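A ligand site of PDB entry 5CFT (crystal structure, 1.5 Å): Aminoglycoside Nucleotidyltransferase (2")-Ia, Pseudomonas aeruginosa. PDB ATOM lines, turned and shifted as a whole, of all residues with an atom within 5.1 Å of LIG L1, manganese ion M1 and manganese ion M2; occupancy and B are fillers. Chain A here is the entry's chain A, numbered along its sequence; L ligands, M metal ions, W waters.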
ATOM      1  N   GLY A  35      -2.553   8.454  15.363  1.00  0.00           N
ATOM      2  CA  GLY A  35      -1.526   7.452  15.395  1.00  0.00           C
ATOM      3  C   GLY A  35      -0.117   7.911  15.083  1.00  0.00           C
ATOM      4  O   GLY A  35       0.293   9.014  15.434  1.00  0.00           O
ATOM      5  N   GLY A  36       0.630   7.080  14.355  1.00  0.00           N
ATOM      6  CA  GLY A  36       2.040   7.339  14.100  1.00  0.00           C
ATOM      7  C   GLY A  36       2.289   8.611  13.361  1.00  0.00           C
ATOM      8  O   GLY A  36       3.234   9.337  13.634  1.00  0.00           O
ATOM      9  N   ASP A  52       0.398   2.602   8.002  1.00  0.00           N
ATOM     10  CA  ASP A  52      -0.893   3.110   7.523  1.00  0.00           C
ATOM     11  C   ASP A  52      -1.064   4.580   7.850  1.00  0.00           C
ATOM     12  O   ASP A  52      -0.146   5.214   8.374  1.00  0.00           O
ATOM     13  CB  ASP A  52      -2.075   2.284   8.091  1.00  0.00           C
ATOM     14  CG  ASP A  52      -2.230   2.378   9.546  1.00  0.00           C
ATOM     15  OD1 ASP A  52      -1.728   3.312  10.145  1.00  0.00           O
ATOM     16  OD2 ASP A  52      -2.957   1.489  10.124  1.00  0.00           O
ATOM     17  N   ILE A  53      -2.210   5.148   7.465  1.00  0.00           N
ATOM     18  CA  ILE A  53      -2.600   6.488   7.806  1.00  0.00           C
ATOM     19  C   ILE A  53      -3.853   6.382   8.662  1.00  0.00           C
ATOM     20  O   ILE A  53      -4.860   5.844   8.190  1.00  0.00           O
ATOM     21  CB  ILE A  53      -2.880   7.279   6.556  1.00  0.00           C
ATOM     22  CG1 ILE A  53      -1.624   7.437   5.665  1.00  0.00           C
ATOM     23  CG2 ILE A  53      -3.366   8.665   6.883  1.00  0.00           C
ATOM     24  CD1 ILE A  53      -1.939   7.828   4.202  1.00  0.00           C
ATOM     25  N   ASP A  54      -3.787   6.791   9.910  1.00  0.00           N
ATOM     26  CA  ASP A  54      -4.898   6.835  10.829  1.00  0.00           C
ATOM     27  C   ASP A  54      -5.604   8.175  10.718  1.00  0.00           C
ATOM     28  O   ASP A  54      -4.964   9.222  10.797  1.00  0.00           O
ATOM     29  CB  ASP A  54      -4.394   6.594  12.248  1.00  0.00           C
ATOM     30  CG  ASP A  54      -3.670   5.280  12.403  1.00  0.00           C
ATOM     31  OD1 ASP A  54      -4.333   4.203  12.358  1.00  0.00           O
ATOM     32  OD2 ASP A  54      -2.420   5.278  12.546  1.00  0.00           O
ATOM     33  N   LEU A  80     -14.605  -2.391  11.062  1.00  0.00           N
ATOM     34  CA  LEU A  80     -14.103  -2.874  12.354  1.00  0.00           C
ATOM     35  C   LEU A  80     -15.036  -2.449  13.444  1.00  0.00           C
ATOM     36  O   LEU A  80     -15.978  -1.682  13.200  1.00  0.00           O
ATOM     37  CB  LEU A  80     -12.714  -2.308  12.664  1.00  0.00           C
ATOM     38  CG  LEU A  80     -11.513  -2.826  11.879  1.00  0.00           C
ATOM     39  CD1 LEU A  80     -11.429  -4.367  11.839  1.00  0.00           C
ATOM     40  CD2 LEU A  80     -11.589  -2.224  10.560  1.00  0.00           C
ATOM     41  N   TYR A  82     -14.593  -0.329  15.682  1.00  0.00           N
ATOM     42  CA  TYR A  82     -14.496   1.081  16.032  1.00  0.00           C
ATOM     43  C   TYR A  82     -14.573   2.015  14.809  1.00  0.00           C
ATOM     44  O   TYR A  82     -14.571   3.247  14.992  1.00  0.00           O
ATOM     45  CB  TYR A  82     -13.152   1.363  16.771  1.00  0.00           C
ATOM     46  CG  TYR A  82     -11.970   1.079  15.842  1.00  0.00           C
ATOM     47  CD1 TYR A  82     -11.531   2.025  14.879  1.00  0.00           C
ATOM     48  CD2 TYR A  82     -11.327  -0.122  15.887  1.00  0.00           C
ATOM     49  CE1 TYR A  82     -10.495   1.693  14.030  1.00  0.00           C
ATOM     50  CE2 TYR A  82     -10.291  -0.444  15.007  1.00  0.00           C
ATOM     51  CZ  TYR A  82      -9.893   0.476  14.114  1.00  0.00           C
ATOM     52  OH  TYR A  82      -8.874   0.105  13.289  1.00  0.00           O
ATOM     53  N   LEU A  85     -11.619   0.355   7.588  1.00  0.00           N
ATOM     54  CA  LEU A  85     -10.371   0.459   6.840  1.00  0.00           C
ATOM     55  C   LEU A  85     -10.771   0.743   5.403  1.00  0.00           C
ATOM     56  O   LEU A  85     -11.793   0.263   4.878  1.00  0.00           O
ATOM     57  CB  LEU A  85      -9.501  -0.808   6.915  1.00  0.00           C
ATOM     58  CG  LEU A  85      -9.213  -1.376   8.315  1.00  0.00           C
ATOM     59  CD1 LEU A  85      -8.361  -2.612   8.085  1.00  0.00           C
ATOM     60  CD2 LEU A  85      -8.444  -0.403   9.183  1.00  0.00           C
ATOM     61  N   LEU A  92      -3.135   1.997   3.153  1.00  0.00           N
ATOM     62  CA  LEU A  92      -4.239   1.760   4.043  1.00  0.00           C
ATOM     63  C   LEU A  92      -4.619   2.956   4.877  1.00  0.00           C
ATOM     64  O   LEU A  92      -3.727   3.604   5.447  1.00  0.00           O
ATOM     65  CB  LEU A  92      -3.891   0.639   4.992  1.00  0.00           C
ATOM     66  CG  LEU A  92      -5.015   0.009   5.738  1.00  0.00           C
ATOM     67  CD1 LEU A  92      -5.796  -0.776   4.698  1.00  0.00           C
ATOM     68  CD2 LEU A  92      -4.347  -0.919   6.765  1.00  0.00           C
ATOM     69  N   ASP A  94      -6.952   3.957   8.121  1.00  0.00           N
ATOM     70  CA  ASP A  94      -7.611   3.358   9.280  1.00  0.00           C
ATOM     71  C   ASP A  94      -8.445   4.439   9.910  1.00  0.00           C
ATOM     72  O   ASP A  94      -7.878   5.377  10.507  1.00  0.00           O
ATOM     73  CB  ASP A  94      -6.536   2.804  10.194  1.00  0.00           C
ATOM     74  CG  ASP A  94      -7.052   2.185  11.431  1.00  0.00           C
ATOM     75  OD1 ASP A  94      -8.254   2.106  11.663  1.00  0.00           O
ATOM     76  OD2 ASP A  94      -6.193   1.675  12.200  1.00  0.00           O
ATOM     77  N   GLU A  96     -11.620   6.282  12.045  1.00  0.00           N
ATOM     78  CA  GLU A  96     -12.481   6.191  13.197  1.00  0.00           C
ATOM     79  C   GLU A  96     -13.329   7.463  13.309  1.00  0.00           C
ATOM     80  O   GLU A  96     -12.819   8.578  13.118  1.00  0.00           O
ATOM     81  CB  GLU A  96     -11.620   6.015  14.467  1.00  0.00           C
ATOM     82  CG  GLU A  96     -12.402   5.911  15.668  1.00  0.00           C
ATOM     83  CD  GLU A  96     -11.616   5.586  16.911  1.00  0.00           C
ATOM     84  OE1 GLU A  96     -10.604   6.196  17.133  1.00  0.00           O
ATOM     85  OE2 GLU A  96     -12.098   4.723  17.701  1.00  0.00           O
ATOM     86  N   ILE A 107     -13.459  12.005  20.071  1.00  0.00           N
ATOM     87  CA  ILE A 107     -13.423  10.551  20.024  1.00  0.00           C
ATOM     88  C   ILE A 107     -14.145  10.024  21.289  1.00  0.00           C
ATOM     89  O   ILE A 107     -13.859  10.481  22.424  1.00  0.00           O
ATOM     90  CB  ILE A 107     -12.008  10.080  19.935  1.00  0.00           C
ATOM     91  CG1 ILE A 107     -11.377  10.461  18.596  1.00  0.00           C
ATOM     92  CG2 ILE A 107     -11.880   8.600  20.190  1.00  0.00           C
ATOM     93  CD1 ILE A 107      -9.855  10.397  18.559  1.00  0.00           C
ATOM     94  N   ALA A 108     -15.024   9.046  21.145  1.00  0.00           N
ATOM     95  CA  ALA A 108     -15.778   8.549  22.283  1.00  0.00           C
ATOM     96  C   ALA A 108     -14.830   8.038  23.336  1.00  0.00           C
ATOM     97  O   ALA A 108     -13.867   7.332  23.046  1.00  0.00           O
ATOM     98  CB  ALA A 108     -16.753   7.480  21.858  1.00  0.00           C
ATOM     99  N   GLU A 109     -15.109   8.434  24.573  1.00  0.00           N
ATOM    100  CA  GLU A 109     -14.399   8.009  25.778  1.00  0.00           C
ATOM    101  C   GLU A 109     -12.958   8.552  25.906  1.00  0.00           C
ATOM    102  O   GLU A 109     -12.280   8.215  26.873  1.00  0.00           O
ATOM    103  CB  GLU A 109     -14.416   6.482  25.870  1.00  0.00           C
ATOM    104  CG  GLU A 109     -15.861   5.896  25.988  1.00  0.00           C
ATOM    105  CD  GLU A 109     -15.885   4.390  26.209  1.00  0.00           C
ATOM    106  OE1 GLU A 109     -16.517   3.680  25.395  1.00  0.00           O
ATOM    107  OE2 GLU A 109     -15.264   3.906  27.173  1.00  0.00           O
ATOM    108  N   ASP A 139      -4.857   6.012  23.448  1.00  0.00           N
ATOM    109  CA  ASP A 139      -5.008   4.765  22.687  1.00  0.00           C
ATOM    110  C   ASP A 139      -3.916   3.764  22.998  1.00  0.00           C
ATOM    111  O   ASP A 139      -4.159   2.575  22.904  1.00  0.00           O
ATOM    112  CB  ASP A 139      -5.073   5.039  21.177  1.00  0.00           C
ATOM    113  CG  ASP A 139      -6.469   5.101  20.628  1.00  0.00           C
ATOM    114  OD1 ASP A 139      -7.419   4.797  21.364  1.00  0.00           O
ATOM    115  OD2 ASP A 139      -6.561   5.439  19.422  1.00  0.00           O
ATOM    116  N   TYR A 142      -5.173   1.688  25.958  1.00  0.00           N
ATOM    117  CA  TYR A 142      -6.021   0.568  25.576  1.00  0.00           C
ATOM    118  C   TYR A 142      -5.156  -0.581  25.054  1.00  0.00           C
ATOM    119  O   TYR A 142      -5.380  -1.724  25.372  1.00  0.00           O
ATOM    120  CB  TYR A 142      -7.011   0.925  24.470  1.00  0.00           C
ATOM    121  CG  TYR A 142      -8.131   1.854  24.832  1.00  0.00           C
ATOM    122  CD1 TYR A 142      -9.111   1.478  25.744  1.00  0.00           C
ATOM    123  CD2 TYR A 142      -8.256   3.078  24.193  1.00  0.00           C
ATOM    124  CE1 TYR A 142     -10.124   2.330  26.038  1.00  0.00           C
ATOM    125  CE2 TYR A 142      -9.278   3.930  24.490  1.00  0.00           C
ATOM    126  CZ  TYR A 142     -10.210   3.530  25.395  1.00  0.00           C
ATOM    127  OH  TYR A 142     -11.223   4.427  25.647  1.00  0.00           O
HETATM  128  O1  LIG L   1      -4.214   0.232  13.706  1.00  0.00           O
HETATM  129  C1  LIG L   1      -4.777  -0.803  14.519  1.00  0.00           C
HETATM  130  C2  LIG L   1      -5.855  -1.558  13.746  1.00  0.00           C
HETATM  131  N1  LIG L   1      -5.336  -2.150  12.518  1.00  0.00           N
HETATM  132  C3  LIG L   1      -6.164  -1.865  11.346  1.00  0.00           C
HETATM  133  C4  LIG L   1      -6.413  -2.671  14.624  1.00  0.00           C
HETATM  134  C5  LIG L   1      -7.580  -3.381  13.955  1.00  0.00           C
HETATM  135  O2  LIG L   1      -5.341  -3.618  14.771  1.00  0.00           O
HETATM  136  C6  LIG L   1      -6.859  -2.097  15.979  1.00  0.00           C
HETATM  137  O3  LIG L   1      -5.844  -1.300  16.589  1.00  0.00           O
HETATM  138  C7  LIG L   1      -5.341  -0.230  15.810  1.00  0.00           C
HETATM  139  O4  LIG L   1      -6.414   0.624  15.529  1.00  0.00           O
HETATM  140  C8  LIG L   1      -6.748   1.680  16.473  1.00  0.00           C
HETATM  141  C9  LIG L   1      -7.412   2.806  15.682  1.00  0.00           C
HETATM  142  N2  LIG L   1      -6.579   3.339  14.581  1.00  0.00           N
HETATM  143  C10 LIG L   1      -7.820   3.931  16.639  1.00  0.00           C
HETATM  144  C11 LIG L   1      -8.784   3.417  17.724  1.00  0.00           C
HETATM  145  N3  LIG L   1      -9.159   4.535  18.625  1.00  0.00           N
HETATM  146  C12 LIG L   1      -7.700   1.156  17.533  1.00  0.00           C
HETATM  147  O5  LIG L   1      -7.053   0.178  18.362  1.00  0.00           O
HETATM  148  C13 LIG L   1      -8.180   2.255  18.473  1.00  0.00           C
HETATM  149  O6  LIG L   1      -9.237   1.691  19.272  1.00  0.00           O
HETATM  150  C14 LIG L   1      -9.253   1.991  20.651  1.00  0.00           C
HETATM  151  C15 LIG L   1      -9.335   0.699  21.475  1.00  0.00           C
HETATM  152  N4  LIG L   1      -8.276  -0.230  21.089  1.00  0.00           N
HETATM  153  C16 LIG L   1     -10.679   0.070  21.192  1.00  0.00           C
HETATM  154  C17 LIG L   1     -11.753   1.070  21.576  1.00  0.00           C
HETATM  155  O7  LIG L   1     -10.275   2.899  20.995  1.00  0.00           O
HETATM  156  C18 LIG L   1     -11.609   2.365  20.805  1.00  0.00           C
HETATM  157  C19 LIG L   1     -12.567   3.450  21.230  1.00  0.00           C
HETATM  158  C20 LIG L   1     -12.472   3.701  22.725  1.00  0.00           C
HETATM  159  N5  LIG L   1     -12.324   4.693  20.482  1.00  0.00           N
HETATM  160  C21 LIG L   1     -13.395   5.654  20.642  1.00  0.00           C
HETATM  161  P1  LG2 L   2       2.278   3.255  11.996  1.00  0.00           P
HETATM  162  O1  LG2 L   2       3.445   2.312  11.528  1.00  0.00           O
HETATM  163  O2  LG2 L   2       0.940   2.722  11.551  1.00  0.00           O
HETATM  164  O3  LG2 L   2       2.504   4.648  11.744  1.00  0.00           O
HETATM  165  P2  LG2 L   2       1.054   3.326  14.542  1.00  0.00           P
HETATM  166  O4  LG2 L   2       1.547   3.787  15.935  1.00  0.00           O
HETATM  167  O5  LG2 L   2       0.093   4.282  13.888  1.00  0.00           O
HETATM  168  O6  LG2 L   2       2.303   3.188  13.613  1.00  0.00           O
HETATM  169  P3  LG2 L   2      -1.254   1.338  14.363  1.00  0.00           P
HETATM  170  O7  LG2 L   2      -1.598  -0.128  14.234  1.00  0.00           O
HETATM  171  O8  LG2 L   2      -1.789   2.171  13.192  1.00  0.00           O
HETATM  172  C1  LG2 L   2       0.466   1.643  14.589  1.00  0.00           C
HETATM  173  O9  LG2 L   2      -2.081   1.771  15.633  1.00  0.00           O
HETATM  174  C2  LG2 L   2      -2.661   3.080  15.865  1.00  0.00           C
HETATM  175  C3  LG2 L   2      -2.695   3.207  17.357  1.00  0.00           C
HETATM  176  O10 LG2 L   2      -3.522   2.155  17.903  1.00  0.00           O
HETATM  177  C4  LG2 L   2      -1.324   3.009  17.958  1.00  0.00           C
HETATM  178  O11 LG2 L   2      -0.747   4.312  18.004  1.00  0.00           O
HETATM  179  C5  LG2 L   2      -1.623   2.372  19.309  1.00  0.00           C
HETATM  180  O12 LG2 L   2      -1.942   3.467  20.161  1.00  0.00           O
HETATM  181  C6  LG2 L   2      -2.875   1.529  19.006  1.00  0.00           C
HETATM  182  N1  LG2 L   2      -2.663   0.084  18.730  1.00  0.00           N
HETATM  183  C7  LG2 L   2      -1.742  -0.529  17.926  1.00  0.00           C
HETATM  184  N2  LG2 L   2      -1.945  -1.820  17.761  1.00  0.00           N
HETATM  185  C8  LG2 L   2      -3.056  -2.077  18.543  1.00  0.00           C
HETATM  186  C9  LG2 L   2      -3.710  -3.274  18.890  1.00  0.00           C
HETATM  187  N3  LG2 L   2      -3.381  -4.478  18.399  1.00  0.00           N
HETATM  188  N4  LG2 L   2      -4.721  -3.208  19.786  1.00  0.00           N
HETATM  189  C10 LG2 L   2      -5.062  -2.025  20.276  1.00  0.00           C
HETATM  190  N5  LG2 L   2      -4.527  -0.826  20.016  1.00  0.00           N
HETATM  191  C11 LG2 L   2      -3.517  -0.916  19.153  1.00  0.00           C
HETATM  192 MN    MN M   1      -0.996   3.828  12.058  1.00  0.00          MN
HETATM  193 MN    MN M   2      -3.903   1.991  12.199  1.00  0.00          MN
HETATM  194  O   HOH W   1      -5.818   1.364  21.064  1.00  0.00           O
HETATM  195  O   HOH W   2      -8.113   5.268  13.344  1.00  0.00           O
HETATM  196  O   HOH W   3      -9.118  -2.209  19.107  1.00  0.00           O
HETATM  197  O   HOH W   4      -4.921  -4.702  11.425  1.00  0.00           O
HETATM  198  O   HOH W   5       0.150   5.534  11.072  1.00  0.00           O
HETATM  199  O   HOH W   6     -15.295   2.337  19.346  1.00  0.00           O
HETATM  200  O   HOH W   7     -11.325   6.580  23.796  1.00  0.00           O
HETATM  201  O   HOH W   8      -5.085   5.589  15.529  1.00  0.00           O
HETATM  202  O   HOH W   9      -2.656  -2.195  12.262  1.00  0.00           O
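OE1 of Glu 96 is in salt-bridge range of N3 of LIG L1 (2.7 Å).
A nitrogen (N3) of LIG L1 lies within salt-bridge range of the side-chain carboxylate of Asp 139 (2.9 Å).
OH of Tyr 82 sits at hydrogen-bond distance from O4 of LIG L1 (3.4 Å).
O5 of LG2 L2 lies close to N of Gly 36.
OD1 of Asp 94 lies within hydrogen-bond range of OH of Tyr 82 (2.7 Å).
The backbone carbonyl oxygen (O) of Ile 53 sits at hydrogen-bond distance from the backbone NH (N) of Asp 94.
Merely in contact with LIG L1: Leu 85 (3.5 Å), Ile 107 (3.3 Å), Ala 108 (3.0 Å) and Tyr 142 (3.3 Å).
Hydrophobic or aromatic side chains within 4 Å of LIG L1: Tyr 82, Leu 85, Ile 107 and Tyr 142.
Within 4 Å of LIG L1: Asp 52, Asp 54, Tyr 82, Leu 85, Asp 94, Glu 96, Ile 107, Ala 108, Asp 139 and Tyr 142.
Two residues have an atom within 4 Å of manganese ion M1: Asp 52 and Asp 54.
Along chain A the residues within 4 Å of manganese ion M1 span positions 52 to 54.
The nearest printed residue that does not touch manganese ion M1 is Gly 36 (4.3 Å).
The nearest printed residue that does not touch manganese ion M2 is Tyr 82 (5.4 Å).
Manganese ion M1 is bound by the side-chain carboxylate of Asp 54, the side-chain carboxylate of Asp 52, an oxygen (O8) of LG2 L2, an oxygen (O5) of LG2 L2, water W5 and an oxygen (O2) of LG2 L2.
Manganese ion M1 has six donor atoms within binding distance.
Manganese ion M2 is bound by OD1 of Asp 54, OD2 of Asp 94, OD2 of Asp 52, O1 of LIG L1 and O8 of LG2 L2.
Manganese ion M2 has five donor atoms within binding distance.
Water W5 lies within hydrogen-bond range of an oxygen (O3) of LG2 L2 and the backbone carbonyl oxygen of Asp 52.
Water W9 bridges N1 of LIG L1 (2.7 Å) and O7 of LG2 L2 (3.0 Å).
Water W2 bridges N2 of LIG L1 (2.8 Å) and O of Asp 94 (2.8 Å).
Water W1 lies within hydrogen-bond range of a nitrogen (N5) of LG2 L2 (2.7 Å), the backbone carbonyl oxygen (O) of Asp 139 (2.8 Å) and a nitrogen (N4) of LIG L1 (2.9 Å).
Water W7 bridges O of Ala 108 (2.8 Å) and OH of Tyr 142 (2.8 Å).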
